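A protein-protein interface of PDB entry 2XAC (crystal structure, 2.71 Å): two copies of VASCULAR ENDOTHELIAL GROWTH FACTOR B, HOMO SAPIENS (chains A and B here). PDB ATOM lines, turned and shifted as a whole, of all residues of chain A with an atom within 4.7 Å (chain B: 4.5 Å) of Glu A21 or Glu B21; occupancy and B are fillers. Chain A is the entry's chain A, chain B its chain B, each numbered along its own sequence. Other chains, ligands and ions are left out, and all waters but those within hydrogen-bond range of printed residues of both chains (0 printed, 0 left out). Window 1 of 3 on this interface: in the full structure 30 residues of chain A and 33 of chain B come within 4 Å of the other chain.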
ATOM      1  N   ARG A  14       0.485  32.306 -20.230  1.00  0.00           N
ATOM      2  CA  ARG A  14       0.158  31.525 -19.049  1.00  0.00           C
ATOM      3  C   ARG A  14       0.779  32.165 -17.805  1.00  0.00           C
ATOM      4  O   ARG A  14       0.125  32.284 -16.768  1.00  0.00           O
ATOM      5  CB  ARG A  14       0.634  30.079 -19.220  1.00  0.00           C
ATOM      6  CG  ARG A  14       0.075  29.110 -18.186  1.00  0.00           C
ATOM      7  CD  ARG A  14       0.652  27.701 -18.337  1.00  0.00           C
ATOM      8  NE  ARG A  14       0.266  26.826 -17.226  1.00  0.00           N
ATOM      9  CZ  ARG A  14       0.548  25.525 -17.153  1.00  0.00           C
ATOM     10  NH1 ARG A  14       1.223  24.918 -18.131  1.00  0.00           N
ATOM     11  NH2 ARG A  14       0.150  24.824 -16.097  1.00  0.00           N
ATOM     12  N   ARG A  20      -5.310  34.776 -10.069  1.00  0.00           N
ATOM     13  CA  ARG A  20      -5.157  33.322 -10.015  1.00  0.00           C
ATOM     14  C   ARG A  20      -5.329  32.756  -8.604  1.00  0.00           C
ATOM     15  O   ARG A  20      -5.217  33.475  -7.614  1.00  0.00           O
ATOM     16  CB  ARG A  20      -3.812  32.899 -10.616  1.00  0.00           C
ATOM     17  CG  ARG A  20      -2.636  33.764 -10.198  1.00  0.00           C
ATOM     18  CD  ARG A  20      -1.403  33.378 -10.974  1.00  0.00           C
ATOM     19  NE  ARG A  20      -1.414  33.868 -12.352  1.00  0.00           N
ATOM     20  CZ  ARG A  20      -0.781  33.274 -13.361  1.00  0.00           C
ATOM     21  NH1 ARG A  20      -0.092  32.154 -13.155  1.00  0.00           N
ATOM     22  NH2 ARG A  20      -0.839  33.790 -14.582  1.00  0.00           N
ATOM     23  N   GLU A  21      -5.599  31.457  -8.528  1.00  0.00           N
ATOM     24  CA  GLU A  21      -5.898  30.807  -7.254  1.00  0.00           C
ATOM     25  C   GLU A  21      -4.674  30.582  -6.374  1.00  0.00           C
ATOM     26  O   GLU A  21      -3.689  29.965  -6.784  1.00  0.00           O
ATOM     27  CB  GLU A  21      -6.712  29.520  -7.460  1.00  0.00           C
ATOM     28  CG  GLU A  21      -6.389  28.736  -8.721  1.00  0.00           C
ATOM     29  CD  GLU A  21      -5.505  27.528  -8.469  1.00  0.00           C
ATOM     30  OE1 GLU A  21      -4.658  27.578  -7.547  1.00  0.00           O
ATOM     31  OE2 GLU A  21      -5.662  26.527  -9.205  1.00  0.00           O
ATOM     32  N   VAL A  22      -4.756  31.127  -5.163  1.00  0.00           N
ATOM     33  CA  VAL A  22      -3.700  31.038  -4.164  1.00  0.00           C
ATOM     34  C   VAL A  22      -4.302  30.614  -2.820  1.00  0.00           C
ATOM     35  O   VAL A  22      -5.268  31.210  -2.339  1.00  0.00           O
ATOM     36  CB  VAL A  22      -2.940  32.385  -4.028  1.00  0.00           C
ATOM     37  CG1 VAL A  22      -2.130  32.446  -2.737  1.00  0.00           C
ATOM     38  CG2 VAL A  22      -2.035  32.611  -5.229  1.00  0.00           C
ATOM     39  N   VAL A  23      -3.726  29.570  -2.233  1.00  0.00           N
ATOM     40  CA  VAL A  23      -4.134  29.080  -0.923  1.00  0.00           C
ATOM     41  C   VAL A  23      -3.770  30.116   0.144  1.00  0.00           C
ATOM     42  O   VAL A  23      -2.681  30.702   0.122  1.00  0.00           O
ATOM     43  CB  VAL A  23      -3.481  27.710  -0.607  1.00  0.00           C
ATOM     44  CG1 VAL A  23      -3.978  27.154   0.716  1.00  0.00           C
ATOM     45  CG2 VAL A  23      -3.754  26.723  -1.728  1.00  0.00           C
ATOM     46  N   THR A  44      -8.892  29.027  -0.762  1.00  0.00           N
ATOM     47  CA  THR A  44      -8.280  29.481  -2.000  1.00  0.00           C
ATOM     48  C   THR A  44      -8.998  30.729  -2.487  1.00  0.00           C
ATOM     49  O   THR A  44     -10.221  30.739  -2.632  1.00  0.00           O
ATOM     50  CB  THR A  44      -8.337  28.408  -3.091  1.00  0.00           C
ATOM     51  OG1 THR A  44      -7.847  27.166  -2.572  1.00  0.00           O
ATOM     52  CG2 THR A  44      -7.486  28.811  -4.269  1.00  0.00           C
ATOM     53  N   VAL A  45      -8.212  31.775  -2.720  1.00  0.00           N
ATOM     54  CA  VAL A  45      -8.694  33.044  -3.243  1.00  0.00           C
ATOM     55  C   VAL A  45      -8.084  33.298  -4.617  1.00  0.00           C
ATOM     56  O   VAL A  45      -7.175  32.578  -5.045  1.00  0.00           O
ATOM     57  CB  VAL A  45      -8.310  34.222  -2.319  1.00  0.00           C
ATOM     58  CG1 VAL A  45      -9.229  34.288  -1.119  1.00  0.00           C
ATOM     59  CG2 VAL A  45      -6.845  34.121  -1.885  1.00  0.00           C
ATOM     60  N   GLN A  46      -8.593  34.327  -5.292  1.00  0.00           N
ATOM     61  CA  GLN A  46      -8.101  34.755  -6.595  1.00  0.00           C
ATOM     62  C   GLN A  46      -7.324  36.047  -6.396  1.00  0.00           C
ATOM     63  O   GLN A  46      -7.859  37.022  -5.881  1.00  0.00           O
ATOM     64  CB  GLN A  46      -9.282  34.976  -7.541  1.00  0.00           C
ATOM     65  CG  GLN A  46      -8.952  34.938  -9.018  1.00  0.00           C
ATOM     66  CD  GLN A  46     -10.095  35.466  -9.871  1.00  0.00           C
ATOM     67  OE1 GLN A  46     -10.757  36.442  -9.508  1.00  0.00           O
ATOM     68  NE2 GLN A  46     -10.332  34.823 -11.015  1.00  0.00           N
ATOM     69  N   ARG B  20      -2.637  22.376  -8.355  1.00  0.00           N
ATOM     70  CA  ARG B  20      -3.118  23.706  -8.720  1.00  0.00           C
ATOM     71  C   ARG B  20      -2.009  24.658  -9.154  1.00  0.00           C
ATOM     72  O   ARG B  20      -0.862  24.529  -8.729  1.00  0.00           O
ATOM     73  CB  ARG B  20      -3.972  24.306  -7.596  1.00  0.00           C
ATOM     74  CG  ARG B  20      -3.229  24.679  -6.328  1.00  0.00           C
ATOM     75  CD  ARG B  20      -4.090  24.410  -5.099  1.00  0.00           C
ATOM     76  NE  ARG B  20      -5.392  25.075  -5.152  1.00  0.00           N
ATOM     77  CZ  ARG B  20      -6.448  24.727  -4.419  1.00  0.00           C
ATOM     78  NH1 ARG B  20      -6.376  23.703  -3.570  1.00  0.00           N
ATOM     79  NH2 ARG B  20      -7.587  25.397  -4.543  1.00  0.00           N
ATOM     80  N   GLU B  21      -2.380  25.616 -10.002  1.00  0.00           N
ATOM     81  CA  GLU B  21      -1.430  26.516 -10.653  1.00  0.00           C
ATOM     82  C   GLU B  21      -0.725  27.470  -9.698  1.00  0.00           C
ATOM     83  O   GLU B  21      -1.363  28.247  -8.985  1.00  0.00           O
ATOM     84  CB  GLU B  21      -2.114  27.297 -11.783  1.00  0.00           C
ATOM     85  CG  GLU B  21      -2.794  26.421 -12.831  1.00  0.00           C
ATOM     86  CD  GLU B  21      -2.004  25.161 -13.156  1.00  0.00           C
ATOM     87  OE1 GLU B  21      -2.492  24.064 -12.816  1.00  0.00           O
ATOM     88  OE2 GLU B  21      -0.900  25.267 -13.734  1.00  0.00           O
ATOM     89  N   VAL B  22       0.601  27.389  -9.700  1.00  0.00           N
ATOM     90  CA  VAL B  22       1.455  28.224  -8.869  1.00  0.00           C
ATOM     91  C   VAL B  22       2.411  29.006  -9.769  1.00  0.00           C
ATOM     92  O   VAL B  22       2.873  28.498 -10.794  1.00  0.00           O
ATOM     93  CB  VAL B  22       2.257  27.369  -7.855  1.00  0.00           C
ATOM     94  CG1 VAL B  22       3.068  28.250  -6.903  1.00  0.00           C
ATOM     95  CG2 VAL B  22       1.324  26.468  -7.063  1.00  0.00           C
ATOM     96  N   VAL B  23       2.685  30.249  -9.387  1.00  0.00           N
ATOM     97  CA  VAL B  23       3.656  31.079 -10.092  1.00  0.00           C
ATOM     98  C   VAL B  23       5.055  30.780  -9.578  1.00  0.00           C
ATOM     99  O   VAL B  23       5.362  31.005  -8.402  1.00  0.00           O
ATOM    100  CB  VAL B  23       3.368  32.585  -9.929  1.00  0.00           C
ATOM    101  CG1 VAL B  23       4.349  33.412 -10.759  1.00  0.00           C
ATOM    102  CG2 VAL B  23       1.951  32.894 -10.339  1.00  0.00           C
ATOM    103  N   THR B  44       4.035  29.456 -14.844  1.00  0.00           N
ATOM    104  CA  THR B  44       2.868  28.872 -14.202  1.00  0.00           C
ATOM    105  C   THR B  44       2.912  27.362 -14.384  1.00  0.00           C
ATOM    106  O   THR B  44       3.085  26.872 -15.505  1.00  0.00           O
ATOM    107  CB  THR B  44       1.568  29.447 -14.790  1.00  0.00           C
ATOM    108  OG1 THR B  44       1.565  30.869 -14.621  1.00  0.00           O
ATOM    109  CG2 THR B  44       0.341  28.864 -14.095  1.00  0.00           C
ATOM    110  N   VAL B  45       2.766  26.631 -13.279  1.00  0.00           N
ATOM    111  CA  VAL B  45       2.851  25.170 -13.303  1.00  0.00           C
ATOM    112  C   VAL B  45       1.925  24.522 -12.261  1.00  0.00           C
ATOM    113  O   VAL B  45       1.703  25.075 -11.187  1.00  0.00           O
ATOM    114  CB  VAL B  45       4.336  24.686 -13.168  1.00  0.00           C
ATOM    115  CG1 VAL B  45       4.862  24.861 -11.747  1.00  0.00           C
ATOM    116  CG2 VAL B  45       4.491  23.254 -13.642  1.00  0.00           C
ATOM    117  N   GLN B  46       1.381  23.358 -12.604  1.00  0.00           N
ATOM    118  CA  GLN B  46       0.434  22.622 -11.762  1.00  0.00           C
ATOM    119  C   GLN B  46       1.179  21.983 -10.582  1.00  0.00           C
ATOM    120  O   GLN B  46       2.079  21.170 -10.784  1.00  0.00           O
ATOM    121  CB  GLN B  46      -0.266  21.552 -12.615  1.00  0.00           C
ATOM    122  CG  GLN B  46      -1.654  21.132 -12.164  1.00  0.00           C
ATOM    123  CD  GLN B  46      -2.295  20.083 -13.083  1.00  0.00           C
ATOM    124  OE1 GLN B  46      -3.521  20.033 -13.223  1.00  0.00           O
ATOM    125  NE2 GLN B  46      -1.464  19.239 -13.708  1.00  0.00           N
ATOM    126  N   GLU B  88       5.752  19.326 -12.739  1.00  0.00           N
ATOM    127  CA  GLU B  88       4.312  19.526 -12.733  1.00  0.00           C
ATOM    128  C   GLU B  88       3.645  18.331 -12.079  1.00  0.00           C
ATOM    129  O   GLU B  88       4.092  17.209 -12.266  1.00  0.00           O
ATOM    130  CB  GLU B  88       3.776  19.730 -14.147  1.00  0.00           C
ATOM    131  CG  GLU B  88       2.320  20.167 -14.166  1.00  0.00           C
ATOM    132  CD  GLU B  88       1.853  20.690 -15.505  1.00  0.00           C
ATOM    133  OE1 GLU B  88       1.283  21.804 -15.538  1.00  0.00           O
ATOM    134  OE2 GLU B  88       2.047  19.990 -16.523  1.00  0.00           O
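Of the 8 printed residues of chain B, 7 touch a printed residue of chain A.
Hydrophobic or aromatic side chains of chain B that line the printed part of chain A: Val B23.
Among the printed residues, Asp or Glu carboxylates within 4 Å of a Lys or Arg side-chain nitrogen of the other chain: Arg A14 with Glu B21, Arg A14 with Glu B88 and Glu A21 with Arg B20.
The side-chain carboxylate (OE2) of Glu B21 lies within salt-bridge range of the guanidinium group (NH2) of Arg A14 (2.6 Å).
OG1 of Thr B44 is in hydrogen-bond range of O of Arg A14, at 2.9 Å.
OE1 of Glu B88 is in salt-bridge range of NH2 of Arg A14 (3.3 Å).
The guanidinium group of Arg A20 sits at hydrogen-bond distance from the side-chain hydroxyl of Thr B44, 2.6 Å away.
OE1 of Glu A21 is in salt-bridge range of NE of Arg B20 (3.5 Å).
OE2 of Glu A21 is in hydrogen-bond range of N of Glu B21 (3.5 Å).
The guanidinium group of Arg B20 sits at hydrogen-bond distance from the side-chain hydroxyl of Thr A44 (2.7 Å).
Arg A20 touches Val B23, but with the chains exchanged Val A23 does not touch Arg B20 (4.1 Å).
Arg A20 touches Thr B44, and with the chains exchanged Thr A44 touches Arg B20.
Glu A21 touches Arg B20, but with the chains exchanged Arg A20 does not touch Glu B21 (5.4 Å).
Glu A21 touches its own counterpart, Glu B21.
Among the printed residues, merely in contact across the chains: Arg A20 with Val B23 (3.4 Å), Arg A14 with Val B45 (3.9 Å) and Arg A14 with Gln B46 (3.98 Å).
The backbone carbonyl oxygen (O) of Arg A14 sits at hydrogen-bond distance from the guanidinium group (NH2) of Arg A20 (2.8 Å).
OE2 of Glu B21 lies within hydrogen-bond range of N of Gln B46.
The backbone NH (N) of Val B22 sits at hydrogen-bond distance from the backbone carbonyl oxygen (O) of Val B45 (3.0 Å).
OE1 of Glu B88 lies close to N of Gln B46 (3.3 Å).
Glu A21 touches two residues of chain B.
Of chain A, only Arg A14 and Glu A21 come within 4 Å of Glu B21.
Of the printed residues of chain A, Arg B20 touches Glu A21 and Thr A44.
Of the printed residues of chain A, Gln B46 touches Arg A14.
Of the printed residues of chain A, Glu B88 touches Arg A14 (3.3 Å).
Val B22 touches none of the printed residues of chain A.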
